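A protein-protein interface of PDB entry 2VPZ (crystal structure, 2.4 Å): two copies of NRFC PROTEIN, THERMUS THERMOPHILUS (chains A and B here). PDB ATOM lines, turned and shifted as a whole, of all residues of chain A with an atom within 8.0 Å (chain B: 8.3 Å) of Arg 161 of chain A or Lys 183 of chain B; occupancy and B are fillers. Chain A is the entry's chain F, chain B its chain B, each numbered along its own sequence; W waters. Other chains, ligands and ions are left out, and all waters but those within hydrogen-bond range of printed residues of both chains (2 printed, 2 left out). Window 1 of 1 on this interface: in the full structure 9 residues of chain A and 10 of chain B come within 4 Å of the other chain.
The backbone carbonyl oxygen (O) of Lys 183 of chain A lies within hydrogen-bond range of the backbone NH (N) of Val 162 of chain B, at 3.0 Å. The side-chain amino group of Lys 183 of chain B lies within hydrogen-bond range of the backbone carbonyl oxygen of Leu 156 of chain A (3.2 Å). The backbone carbonyl oxygen (O) of Lys 157 of chain A sits at hydrogen-bond distance from the side-chain amino group (NZ) of Lys 183 of chain B (2.6 Å). O of Ala 159 of chain A sits at hydrogen-bond distance from NZ of Lys 183 of chain B (2.8 Å). The backbone carbonyl oxygen of Lys 183 of chain B sits at hydrogen-bond distance from the backbone NH of Val 162 of chain A, at 3.0 Å. The guanidinium group (NH2) of Arg 161 of chain B lies close to the guanidinium group (NH2) of Arg 161 of chain A (3.3 Å).
OD2 of Asp 163 of chain B is in salt-bridge range of NE of Arg 161 of chain B (3.1 Å). ND2 of Asn 179 of chain A lies close to N of Glu 160 of chain A, at 2.8 Å. NE of Arg 161 of chain A is in salt-bridge range of OD2 of Asp 163 of chain A (3.1 Å). The side-chain amide nitrogen of Asn 179 of chain A lies close to the backbone NH of Arg 161 of chain A (3.4 Å). The guanidinium group (NH1) of Arg 161 of chain A lies within hydrogen-bond range of the backbone carbonyl oxygen (O) of Lys 183 of chain A. OG of Ser 182 of chain A sits close to N of Lys 184 of chain A, at 3.5 Å.
Asn 48 of chain B touches Lys 157 of chain A. Glu 160 of chain A touches Lys 183 of chain B. Arg 161 of chain A touches Lys 183 of chain B (CA to O, 3.6 Å). O of Val 162 of chain A touches CA of Lys 184 of chain B, 3.6 Å away. Glu 160 of chain B touches Lys 183 of chain A. O of Lys 183 of chain A touches CA of Arg 161 of chain B, at 3.7 Å. Lys 184 of chain A touches Val 162 of chain B.
Printed residues of chain B within 4 Å of Ala 159 of chain A: Lys 183 (2.8 Å). Printed residues of chain B within 4 Å of Glu 160 of chain A: Lys 183. Arg 161 of chain A touches just these residues of chain B: Arg 161 (3.3 Å) and Lys 183 (3.6 Å). Of the printed residues of chain B, Val 162 of chain A touches Lys 183 (3.0 Å) and Lys 184 (3.6 Å). Printed residues of chain B within 4 Å of Lys 184 of chain A: Val 162 (3.7 Å). Of the printed residues of chain A, Asn 48 of chain B touches Lys 157. Ala 180 of chain B touches none of the printed residues of chain A. No residue of chain A comes within 4 Å of Ser 182 of chain B. Of chain A, only Leu 156 (3.2 Å), Lys 157 (2.6 Å), Ala 159 (2.8 Å), Glu 160 (3.7 Å), Arg 161 (3.6 Å) and Val 162 (3.0 Å) come within 4 Å of Lys 183 of chain B.
Printed residues of chain A that touch a printed residue of chain B: Leu 156, Lys 157, Ala 159, Glu 160, Arg 161, Val 162, Lys 183 and Lys 184. Among the printed residues, 13 pairs touch across the chains. Among the printed residues, no Asp or Glu carboxylate lies within 4 Å of a Lys or Arg side-chain nitrogen of the other chain.
Glu 160 of chain A touches Lys 183 of chain B, and with the chains exchanged Lys 183 of chain A touches Glu 160 of chain B. Arg 161 of chain A touches Lys 183 of chain B, and with the chains exchanged Lys 183 of chain A touches Arg 161 of chain B. Val 162 of chain A touches Lys 183 of chain B, and with the chains exchanged Lys 183 of chain A touches Val 162 of chain B. Val 162 of chain A touches Lys 184 of chain B, and with the chains exchanged Lys 184 of chain A touches Val 162 of chain B. Positions printed for both chains: 160, 161, 162, 163, 180, 181, 182, 183, 184, 185 and 186.
Water W1 lies within hydrogen-bond range of NH1 of Arg 161 of chain A (2.7 Å) and O of Glu 160 of chain B (2.7 Å). Water W2 bridges the backbone carbonyl oxygen (O) of Glu 160 of chain A and the guanidinium group (NH1) of Arg 161 of chain B.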
ATOM      1  N   ILE A   8      27.345   8.455   0.954  1.00  0.00           N
ATOM      2  CA  ILE A   8      28.577   8.105   0.266  1.00  0.00           C
ATOM      3  C   ILE A   8      28.606   8.715  -1.124  1.00  0.00           C
ATOM      4  O   ILE A   8      27.771   8.420  -1.974  1.00  0.00           O
ATOM      5  CB  ILE A   8      28.785   6.575   0.187  1.00  0.00           C
ATOM      6  CG1 ILE A   8      28.744   6.000   1.598  1.00  0.00           C
ATOM      7  CG2 ILE A   8      30.171   6.264  -0.410  1.00  0.00           C
ATOM      8  CD1 ILE A   8      28.705   4.474   1.695  1.00  0.00           C
ATOM      9  N   ASP A   9      29.568   9.598  -1.337  1.00  0.00           N
ATOM     10  CA  ASP A   9      29.719  10.283  -2.611  1.00  0.00           C
ATOM     11  C   ASP A   9      30.507   9.355  -3.550  1.00  0.00           C
ATOM     12  O   ASP A   9      31.715   9.283  -3.427  1.00  0.00           O
ATOM     13  CB  ASP A   9      30.456  11.616  -2.378  1.00  0.00           C
ATOM     14  CG  ASP A   9      30.617  12.448  -3.648  1.00  0.00           C
ATOM     15  OD1 ASP A   9      30.381  11.892  -4.741  1.00  0.00           O
ATOM     16  OD2 ASP A   9      30.985  13.643  -3.525  1.00  0.00           O
ATOM     17  N   LEU A  10      29.824   8.645  -4.458  1.00  0.00           N
ATOM     18  CA  LEU A  10      30.450   7.688  -5.396  1.00  0.00           C
ATOM     19  C   LEU A  10      31.340   8.350  -6.481  1.00  0.00           C
ATOM     20  O   LEU A  10      32.110   7.663  -7.171  1.00  0.00           O
ATOM     21  CB  LEU A  10      29.402   6.739  -6.063  1.00  0.00           C
ATOM     22  CG  LEU A  10      28.438   5.880  -5.184  1.00  0.00           C
ATOM     23  CD1 LEU A  10      27.467   5.002  -6.050  1.00  0.00           C
ATOM     24  CD2 LEU A  10      29.271   5.004  -4.203  1.00  0.00           C
ATOM     25  N   ALA A 153      23.394  16.042   5.969  1.00  0.00           N
ATOM     26  CA  ALA A 153      22.428  17.047   5.521  1.00  0.00           C
ATOM     27  C   ALA A 153      22.940  18.030   4.466  1.00  0.00           C
ATOM     28  O   ALA A 153      22.237  18.364   3.506  1.00  0.00           O
ATOM     29  CB  ALA A 153      21.877  17.831   6.742  1.00  0.00           C
ATOM     30  N   LYS A 154      24.167  18.491   4.662  1.00  0.00           N
ATOM     31  CA  LYS A 154      24.832  19.432   3.768  1.00  0.00           C
ATOM     32  C   LYS A 154      25.249  18.782   2.445  1.00  0.00           C
ATOM     33  O   LYS A 154      25.236  19.424   1.383  1.00  0.00           O
ATOM     34  CB  LYS A 154      26.061  20.048   4.433  1.00  0.00           C
ATOM     35  CG  LYS A 154      25.777  21.134   5.438  1.00  0.00           C
ATOM     36  CD  LYS A 154      26.988  22.029   5.552  1.00  0.00           C
ATOM     37  CE  LYS A 154      27.994  21.460   6.530  1.00  0.00           C
ATOM     38  NZ  LYS A 154      27.959  22.259   7.797  1.00  0.00           N
ATOM     39  N   ALA A 155      25.621  17.510   2.526  1.00  0.00           N
ATOM     40  CA  ALA A 155      26.048  16.713   1.372  1.00  0.00           C
ATOM     41  C   ALA A 155      24.832  16.317   0.512  1.00  0.00           C
ATOM     42  O   ALA A 155      24.874  16.404  -0.729  1.00  0.00           O
ATOM     43  CB  ALA A 155      26.830  15.475   1.843  1.00  0.00           C
ATOM     44  N   LEU A 156      23.759  15.878   1.163  1.00  0.00           N
ATOM     45  CA  LEU A 156      22.525  15.575   0.451  1.00  0.00           C
ATOM     46  C   LEU A 156      22.171  16.884  -0.314  1.00  0.00           C
ATOM     47  O   LEU A 156      21.947  16.853  -1.528  1.00  0.00           O
ATOM     48  CB  LEU A 156      21.403  15.142   1.431  1.00  0.00           C
ATOM     49  CG  LEU A 156      21.432  13.677   1.911  1.00  0.00           C
ATOM     50  CD1 LEU A 156      20.550  13.478   3.138  1.00  0.00           C
ATOM     51  CD2 LEU A 156      20.968  12.728   0.790  1.00  0.00           C
ATOM     52  N   LYS A 157      22.168  18.037   0.357  1.00  0.00           N
ATOM     53  CA  LYS A 157      21.865  19.299  -0.340  1.00  0.00           C
ATOM     54  C   LYS A 157      22.780  19.620  -1.529  1.00  0.00           C
ATOM     55  O   LYS A 157      22.314  20.155  -2.532  1.00  0.00           O
ATOM     56  CB  LYS A 157      21.870  20.526   0.590  1.00  0.00           C
ATOM     57  CG  LYS A 157      20.655  20.647   1.505  1.00  0.00           C
ATOM     58  CD  LYS A 157      19.321  20.744   0.731  1.00  0.00           C
ATOM     59  CE  LYS A 157      18.129  20.846   1.697  1.00  0.00           C
ATOM     60  NZ  LYS A 157      18.498  21.640   2.922  1.00  0.00           N
ATOM     61  N   ALA A 158      24.068  19.308  -1.430  1.00  0.00           N
ATOM     62  CA  ALA A 158      25.019  19.602  -2.512  1.00  0.00           C
ATOM     63  C   ALA A 158      25.063  18.581  -3.665  1.00  0.00           C
ATOM     64  O   ALA A 158      25.586  18.877  -4.746  1.00  0.00           O
ATOM     65  CB  ALA A 158      26.453  19.811  -1.932  1.00  0.00           C
ATOM     66  N   ALA A 159      24.509  17.395  -3.447  1.00  0.00           N
ATOM     67  CA  ALA A 159      24.511  16.350  -4.471  1.00  0.00           C
ATOM     68  C   ALA A 159      23.780  16.725  -5.758  1.00  0.00           C
ATOM     69  O   ALA A 159      22.795  17.457  -5.741  1.00  0.00           O
ATOM     70  CB  ALA A 159      23.927  15.021  -3.907  1.00  0.00           C
ATOM     71  N   GLU A 160      24.303  16.229  -6.870  1.00  0.00           N
ATOM     72  CA  GLU A 160      23.729  16.435  -8.187  1.00  0.00           C
ATOM     73  C   GLU A 160      22.587  15.377  -8.305  1.00  0.00           C
ATOM     74  O   GLU A 160      21.550  15.646  -8.916  1.00  0.00           O
ATOM     75  CB  GLU A 160      24.826  16.251  -9.273  1.00  0.00           C
ATOM     76  CG  GLU A 160      24.804  17.220 -10.499  1.00  0.00           C
ATOM     77  CD  GLU A 160      24.620  18.736 -10.153  1.00  0.00           C
ATOM     78  OE1 GLU A 160      25.308  19.240  -9.226  1.00  0.00           O
ATOM     79  OE2 GLU A 160      23.794  19.420 -10.830  1.00  0.00           O
ATOM     80  N   ARG A 161      22.768  14.204  -7.695  1.00  0.00           N
ATOM     81  CA  ARG A 161      21.778  13.111  -7.712  1.00  0.00           C
ATOM     82  C   ARG A 161      21.861  12.222  -6.444  1.00  0.00           C
ATOM     83  O   ARG A 161      22.935  12.091  -5.864  1.00  0.00           O
ATOM     84  CB  ARG A 161      21.930  12.267  -9.001  1.00  0.00           C
ATOM     85  CG  ARG A 161      23.236  11.463  -9.168  1.00  0.00           C
ATOM     86  CD  ARG A 161      23.149  10.479 -10.395  1.00  0.00           C
ATOM     87  NE  ARG A 161      22.057   9.490 -10.342  1.00  0.00           N
ATOM     88  CZ  ARG A 161      21.429   8.975 -11.405  1.00  0.00           C
ATOM     89  NH1 ARG A 161      21.773   9.357 -12.623  1.00  0.00           N
ATOM     90  NH2 ARG A 161      20.463   8.059 -11.268  1.00  0.00           N
ATOM     91  N   VAL A 162      20.750  11.634  -6.004  1.00  0.00           N
ATOM     92  CA  VAL A 162      20.704  10.790  -4.798  1.00  0.00           C
ATOM     93  C   VAL A 162      20.001   9.456  -5.102  1.00  0.00           C
ATOM     94  O   VAL A 162      18.922   9.453  -5.704  1.00  0.00           O
ATOM     95  CB  VAL A 162      19.957  11.533  -3.631  1.00  0.00           C
ATOM     96  CG1 VAL A 162      20.003  10.709  -2.352  1.00  0.00           C
ATOM     97  CG2 VAL A 162      20.580  12.914  -3.398  1.00  0.00           C
ATOM     98  N   ASP A 163      20.603   8.340  -4.707  1.00  0.00           N
ATOM     99  CA  ASP A 163      20.055   7.015  -4.977  1.00  0.00           C
ATOM    100  C   ASP A 163      20.113   6.095  -3.747  1.00  0.00           C
ATOM    101  O   ASP A 163      20.813   6.378  -2.760  1.00  0.00           O
ATOM    102  CB  ASP A 163      20.790   6.344  -6.166  1.00  0.00           C
ATOM    103  CG  ASP A 163      20.766   7.174  -7.478  1.00  0.00           C
ATOM    104  OD1 ASP A 163      20.026   6.796  -8.413  1.00  0.00           O
ATOM    105  OD2 ASP A 163      21.496   8.190  -7.576  1.00  0.00           O
ATOM    106  N   PHE A 176      22.650   6.773   1.833  1.00  0.00           N
ATOM    107  CA  PHE A 176      22.435   7.425   0.549  1.00  0.00           C
ATOM    108  C   PHE A 176      23.658   7.500  -0.334  1.00  0.00           C
ATOM    109  O   PHE A 176      24.704   7.975   0.094  1.00  0.00           O
ATOM    110  CB  PHE A 176      21.911   8.847   0.807  1.00  0.00           C
ATOM    111  CG  PHE A 176      20.652   8.904   1.654  1.00  0.00           C
ATOM    112  CD1 PHE A 176      20.717   9.073   3.049  1.00  0.00           C
ATOM    113  CD2 PHE A 176      19.399   8.754   1.051  1.00  0.00           C
ATOM    114  CE1 PHE A 176      19.546   9.096   3.826  1.00  0.00           C
ATOM    115  CE2 PHE A 176      18.214   8.774   1.806  1.00  0.00           C
ATOM    116  CZ  PHE A 176      18.279   8.941   3.192  1.00  0.00           C
ATOM    117  N   TYR A 177      23.529   7.039  -1.567  1.00  0.00           N
ATOM    118  CA  TYR A 177      24.651   7.074  -2.477  1.00  0.00           C
ATOM    119  C   TYR A 177      24.563   8.365  -3.220  1.00  0.00           C
ATOM    120  O   TYR A 177      23.561   8.622  -3.891  1.00  0.00           O
ATOM    121  CB  TYR A 177      24.615   5.884  -3.443  1.00  0.00           C
ATOM    122  CG  TYR A 177      24.917   4.572  -2.753  1.00  0.00           C
ATOM    123  CD1 TYR A 177      23.917   3.632  -2.522  1.00  0.00           C
ATOM    124  CD2 TYR A 177      26.213   4.277  -2.316  1.00  0.00           C
ATOM    125  CE1 TYR A 177      24.192   2.414  -1.873  1.00  0.00           C
ATOM    126  CE2 TYR A 177      26.513   3.063  -1.660  1.00  0.00           C
ATOM    127  CZ  TYR A 177      25.493   2.128  -1.444  1.00  0.00           C
ATOM    128  OH  TYR A 177      25.767   0.925  -0.824  1.00  0.00           O
ATOM    129  N   LEU A 178      25.580   9.198  -3.125  1.00  0.00           N
ATOM    130  CA  LEU A 178      25.431  10.411  -3.837  1.00  0.00           C
ATOM    131  C   LEU A 178      25.713  10.283  -5.332  1.00  0.00           C
ATOM    132  O   LEU A 178      25.138   9.380  -5.981  1.00  0.00           O
ATOM    133  CB  LEU A 178      26.115  11.593  -3.118  1.00  0.00           C
ATOM    134  CG  LEU A 178      25.543  11.574  -1.669  1.00  0.00           C
ATOM    135  CD1 LEU A 178      26.242  12.607  -0.801  1.00  0.00           C
ATOM    136  CD2 LEU A 178      23.997  11.788  -1.613  1.00  0.00           C
ATOM    137  N   ASN A 179      26.604  11.092  -5.868  1.00  0.00           N
ATOM    138  CA  ASN A 179      26.794  11.172  -7.309  1.00  0.00           C
ATOM    139  C   ASN A 179      27.168   9.977  -8.178  1.00  0.00           C
ATOM    140  O   ASN A 179      28.263   9.936  -8.723  1.00  0.00           O
ATOM    141  CB  ASN A 179      27.706  12.369  -7.597  1.00  0.00           C
ATOM    142  CG  ASN A 179      27.287  13.615  -6.815  1.00  0.00           C
ATOM    143  OD1 ASN A 179      27.983  14.064  -5.900  1.00  0.00           O
ATOM    144  ND2 ASN A 179      26.123  14.152  -7.149  1.00  0.00           N
ATOM    145  N   ALA A 180      26.215   9.053  -8.346  1.00  0.00           N
ATOM    146  CA  ALA A 180      26.367   7.815  -9.128  1.00  0.00           C
ATOM    147  C   ALA A 180      27.030   8.060 -10.472  1.00  0.00           C
ATOM    148  O   ALA A 180      26.579   8.925 -11.228  1.00  0.00           O
ATOM    149  CB  ALA A 180      24.988   7.112  -9.343  1.00  0.00           C
ATOM    150  N   PRO A 181      28.098   7.295 -10.800  1.00  0.00           N
ATOM    151  CA  PRO A 181      28.823   7.435 -12.065  1.00  0.00           C
ATOM    152  C   PRO A 181      28.095   7.066 -13.399  1.00  0.00           C
ATOM    153  O   PRO A 181      28.340   7.684 -14.436  1.00  0.00           O
ATOM    154  CB  PRO A 181      30.095   6.623 -11.834  1.00  0.00           C
ATOM    155  CG  PRO A 181      29.605   5.502 -10.947  1.00  0.00           C
ATOM    156  CD  PRO A 181      28.738   6.282  -9.957  1.00  0.00           C
ATOM    157  N   SER A 182      27.236   6.056 -13.418  1.00  0.00           N
ATOM    158  CA  SER A 182      26.517   5.757 -14.666  1.00  0.00           C
ATOM    159  C   SER A 182      25.205   6.586 -14.722  1.00  0.00           C
ATOM    160  O   SER A 182      24.520   6.731 -13.714  1.00  0.00           O
ATOM    161  CB  SER A 182      26.215   4.246 -14.812  1.00  0.00           C
ATOM    162  OG  SER A 182      25.226   3.984 -15.794  1.00  0.00           O
ATOM    163  N   LYS A 183      24.895   7.150 -15.890  1.00  0.00           N
ATOM    164  CA  LYS A 183      23.681   7.946 -16.175  1.00  0.00           C
ATOM    165  C   LYS A 183      22.340   7.251 -15.876  1.00  0.00           C
ATOM    166  O   LYS A 183      21.292   7.904 -15.701  1.00  0.00           O
ATOM    167  CB  LYS A 183      23.639   8.313 -17.635  1.00  0.00           C
ATOM    168  CG  LYS A 183      24.437   9.449 -18.045  1.00  0.00           C
ATOM    169  CD  LYS A 183      24.075   9.645 -19.467  1.00  0.00           C
ATOM    170  CE  LYS A 183      24.991  10.602 -20.147  1.00  0.00           C
ATOM    171  NZ  LYS A 183      24.757  10.540 -21.616  1.00  0.00           N
ATOM    172  N   LYS A 184      22.362   5.926 -15.903  1.00  0.00           N
ATOM    173  CA  LYS A 184      21.160   5.172 -15.614  1.00  0.00           C
ATOM    174  C   LYS A 184      21.033   4.899 -14.128  1.00  0.00           C
ATOM    175  O   LYS A 184      20.085   4.250 -13.710  1.00  0.00           O
ATOM    176  CB  LYS A 184      21.115   3.850 -16.380  1.00  0.00           C
ATOM    177  CG  LYS A 184      21.052   4.043 -17.870  1.00  0.00           C
ATOM    178  CD  LYS A 184      21.107   2.733 -18.628  1.00  0.00           C
ATOM    179  CE  LYS A 184      21.190   2.973 -20.141  1.00  0.00           C
ATOM    180  NZ  LYS A 184      19.863   3.299 -20.800  1.00  0.00           N
ATOM    181  N   GLY A 185      21.973   5.377 -13.327  1.00  0.00           N
ATOM    182  CA  GLY A 185      21.900   5.134 -11.903  1.00  0.00           C
ATOM    183  C   GLY A 185      22.734   3.961 -11.416  1.00  0.00           C
ATOM    184  O   GLY A 185      23.621   3.495 -12.147  1.00  0.00           O
ATOM    185  N   LEU A 186      22.460   3.507 -10.189  1.00  0.00           N
ATOM    186  CA  LEU A 186      23.139   2.388  -9.569  1.00  0.00           C
ATOM    187  C   LEU A 186      22.955   1.127 -10.391  1.00  0.00           C
ATOM    188  O   LEU A 186      21.866   0.758 -10.827  1.00  0.00           O
ATOM    189  CB  LEU A 186      22.646   2.144  -8.131  1.00  0.00           C
ATOM    190  CG  LEU A 186      22.649   3.323  -7.158  1.00  0.00           C
ATOM    191  CD1 LEU A 186      22.267   2.787  -5.794  1.00  0.00           C
ATOM    192  CD2 LEU A 186      24.022   4.047  -7.096  1.00  0.00           C
ATOM    193  N   VAL B  43       7.016  18.485  -5.822  1.00  0.00           N
ATOM    194  CA  VAL B  43       7.852  17.864  -4.827  1.00  0.00           C
ATOM    195  C   VAL B  43       8.494  18.902  -3.887  1.00  0.00           C
ATOM    196  O   VAL B  43       9.288  19.710  -4.335  1.00  0.00           O
ATOM    197  CB  VAL B  43       9.041  17.073  -5.523  1.00  0.00           C
ATOM    198  CG1 VAL B  43       9.750  16.185  -4.484  1.00  0.00           C
ATOM    199  CG2 VAL B  43       8.552  16.243  -6.723  1.00  0.00           C
ATOM    200  N   ASN B  48      13.309  24.707  -1.814  1.00  0.00           N
ATOM    201  CA  ASN B  48      13.645  23.506  -2.621  1.00  0.00           C
ATOM    202  C   ASN B  48      12.300  22.934  -3.196  1.00  0.00           C
ATOM    203  O   ASN B  48      11.863  21.839  -2.793  1.00  0.00           O
ATOM    204  CB  ASN B  48      14.302  22.410  -1.748  1.00  0.00           C
ATOM    205  CG  ASN B  48      15.285  22.957  -0.700  1.00  0.00           C
ATOM    206  OD1 ASN B  48      16.054  23.872  -0.980  1.00  0.00           O
ATOM    207  ND2 ASN B  48      15.275  22.366   0.504  1.00  0.00           N
ATOM    208  N   VAL B  50      10.358  21.695  -6.505  1.00  0.00           N
ATOM    209  CA  VAL B  50      10.533  21.191  -7.850  1.00  0.00           C
ATOM    210  C   VAL B  50       9.184  20.777  -8.456  1.00  0.00           C
ATOM    211  O   VAL B  50       8.326  20.268  -7.723  1.00  0.00           O
ATOM    212  CB  VAL B  50      11.525  19.959  -7.797  1.00  0.00           C
ATOM    213  CG1 VAL B  50      11.508  19.177  -9.109  1.00  0.00           C
ATOM    214  CG2 VAL B  50      12.960  20.432  -7.433  1.00  0.00           C
ATOM    215  N   GLU B 160      22.380  14.396 -19.007  1.00  0.00           N
ATOM    216  CA  GLU B 160      22.985  14.400 -17.660  1.00  0.00           C
ATOM    217  C   GLU B 160      22.483  13.094 -16.892  1.00  0.00           C
ATOM    218  O   GLU B 160      23.232  12.467 -16.139  1.00  0.00           O
ATOM    219  CB  GLU B 160      22.586  15.696 -16.927  1.00  0.00           C
ATOM    220  CG  GLU B 160      23.694  16.400 -16.126  1.00  0.00           C
ATOM    221  CD  GLU B 160      24.836  17.000 -16.989  1.00  0.00           C
ATOM    222  OE1 GLU B 160      24.534  17.816 -17.902  1.00  0.00           O
ATOM    223  OE2 GLU B 160      26.027  16.658 -16.731  1.00  0.00           O
ATOM    224  N   ARG B 161      21.222  12.702 -17.066  1.00  0.00           N
ATOM    225  CA  ARG B 161      20.711  11.446 -16.487  1.00  0.00           C
ATOM    226  C   ARG B 161      19.655  10.833 -17.423  1.00  0.00           C
ATOM    227  O   ARG B 161      19.068  11.548 -18.238  1.00  0.00           O
ATOM    228  CB  ARG B 161      20.111  11.619 -15.069  1.00  0.00           C
ATOM    229  CG  ARG B 161      18.868  12.513 -14.928  1.00  0.00           C
ATOM    230  CD  ARG B 161      18.497  12.671 -13.437  1.00  0.00           C
ATOM    231  NE  ARG B 161      18.078  11.402 -12.843  1.00  0.00           N
ATOM    232  CZ  ARG B 161      18.117  11.078 -11.550  1.00  0.00           C
ATOM    233  NH1 ARG B 161      18.571  11.935 -10.645  1.00  0.00           N
ATOM    234  NH2 ARG B 161      17.694   9.869 -11.158  1.00  0.00           N
ATOM    235  N   VAL B 162      19.448   9.523 -17.342  1.00  0.00           N
ATOM    236  CA  VAL B 162      18.429   8.820 -18.135  1.00  0.00           C
ATOM    237  C   VAL B 162      17.564   7.907 -17.207  1.00  0.00           C
ATOM    238  O   VAL B 162      18.116   7.169 -16.388  1.00  0.00           O
ATOM    239  CB  VAL B 162      19.053   7.963 -19.287  1.00  0.00           C
ATOM    240  CG1 VAL B 162      17.937   7.276 -20.071  1.00  0.00           C
ATOM    241  CG2 VAL B 162      19.909   8.852 -20.220  1.00  0.00           C
ATOM    242  N   ASP B 163      16.231   8.007 -17.314  1.00  0.00           N
ATOM    243  CA  ASP B 163      15.248   7.225 -16.521  1.00  0.00           C
ATOM    244  C   ASP B 163      14.070   6.645 -17.333  1.00  0.00           C
ATOM    245  O   ASP B 163      13.712   7.131 -18.406  1.00  0.00           O
ATOM    246  CB  ASP B 163      14.685   8.023 -15.325  1.00  0.00           C
ATOM    247  CG  ASP B 163      15.780   8.613 -14.416  1.00  0.00           C
ATOM    248  OD1 ASP B 163      16.215   7.968 -13.431  1.00  0.00           O
ATOM    249  OD2 ASP B 163      16.196   9.745 -14.719  1.00  0.00           O
ATOM    250  N   ALA B 180      15.716  14.452 -15.521  1.00  0.00           N
ATOM    251  CA  ALA B 180      14.631  14.638 -14.544  1.00  0.00           C
ATOM    252  C   ALA B 180      14.954  15.740 -13.516  1.00  0.00           C
ATOM    253  O   ALA B 180      16.058  15.752 -12.964  1.00  0.00           O
ATOM    254  CB  ALA B 180      14.356  13.317 -13.796  1.00  0.00           C
ATOM    255  N   PRO B 181      13.987  16.653 -13.236  1.00  0.00           N
ATOM    256  CA  PRO B 181      14.078  17.781 -12.293  1.00  0.00           C
ATOM    257  C   PRO B 181      14.439  17.434 -10.834  1.00  0.00           C
ATOM    258  O   PRO B 181      15.224  18.142 -10.198  1.00  0.00           O
ATOM    259  CB  PRO B 181      12.712  18.478 -12.401  1.00  0.00           C
ATOM    260  CG  PRO B 181      11.803  17.436 -12.991  1.00  0.00           C
ATOM    261  CD  PRO B 181      12.690  16.641 -13.915  1.00  0.00           C
ATOM    262  N   SER B 182      13.868  16.357 -10.298  1.00  0.00           N
ATOM    263  CA  SER B 182      14.154  15.927  -8.914  1.00  0.00           C
ATOM    264  C   SER B 182      15.435  15.056  -8.766  1.00  0.00           C
ATOM    265  O   SER B 182      15.609  14.119  -9.541  1.00  0.00           O
ATOM    266  CB  SER B 182      12.967  15.159  -8.314  1.00  0.00           C
ATOM    267  OG  SER B 182      13.293  14.739  -7.008  1.00  0.00           O
ATOM    268  N   LYS B 183      16.304  15.346  -7.783  1.00  0.00           N
ATOM    269  CA  LYS B 183      17.568  14.588  -7.541  1.00  0.00           C
ATOM    270  C   LYS B 183      17.396  13.075  -7.352  1.00  0.00           C
ATOM    271  O   LYS B 183      18.297  12.288  -7.680  1.00  0.00           O
ATOM    272  CB  LYS B 183      18.311  15.049  -6.289  1.00  0.00           C
ATOM    273  CG  LYS B 183      19.026  16.350  -6.310  1.00  0.00           C
ATOM    274  CD  LYS B 183      19.582  16.585  -4.925  1.00  0.00           C
ATOM    275  CE  LYS B 183      19.608  18.062  -4.625  1.00  0.00           C
ATOM    276  NZ  LYS B 183      20.873  18.547  -3.976  1.00  0.00           N
ATOM    277  N   LYS B 184      16.257  12.696  -6.775  1.00  0.00           N
ATOM    278  CA  LYS B 184      15.893  11.307  -6.494  1.00  0.00           C
ATOM    279  C   LYS B 184      15.261  10.592  -7.676  1.00  0.00           C
ATOM    280  O   LYS B 184      14.900   9.419  -7.579  1.00  0.00           O
ATOM    281  CB  LYS B 184      14.941  11.237  -5.301  1.00  0.00           C
ATOM    282  CG  LYS B 184      15.538  11.719  -4.008  1.00  0.00           C
ATOM    283  CD  LYS B 184      14.444  12.026  -3.008  1.00  0.00           C
ATOM    284  CE  LYS B 184      15.014  12.384  -1.635  1.00  0.00           C
ATOM    285  NZ  LYS B 184      15.663  11.212  -0.936  1.00  0.00           N
ATOM    286  N   GLY B 185      15.103  11.308  -8.773  1.00  0.00           N
ATOM    287  CA  GLY B 185      14.535  10.720  -9.974  1.00  0.00           C
ATOM    288  C   GLY B 185      13.053  10.893 -10.290  1.00  0.00           C
ATOM    289  O   GLY B 185      12.385  11.759  -9.722  1.00  0.00           O
ATOM    290  N   LEU B 186      12.537  10.078 -11.204  1.00  0.00           N
ATOM    291  CA  LEU B 186      11.138  10.171 -11.560  1.00  0.00           C
ATOM    292  C   LEU B 186      10.291  10.021 -10.291  1.00  0.00           C
ATOM    293  O   LEU B 186      10.579   9.231  -9.398  1.00  0.00           O
ATOM    294  CB  LEU B 186      10.754   9.118 -12.634  1.00  0.00           C
ATOM    295  CG  LEU B 186      11.571   9.259 -13.939  1.00  0.00           C
ATOM    296  CD1 LEU B 186      11.301   8.095 -14.895  1.00  0.00           C
ATOM    297  CD2 LEU B 186      11.260  10.587 -14.646  1.00  0.00           C
HETATM  298  O   HOH W   1      23.450  11.148 -13.756  1.00  0.00           O
HETATM  299  O   HOH W   2      19.925  14.648 -10.890  1.00  0.00           O
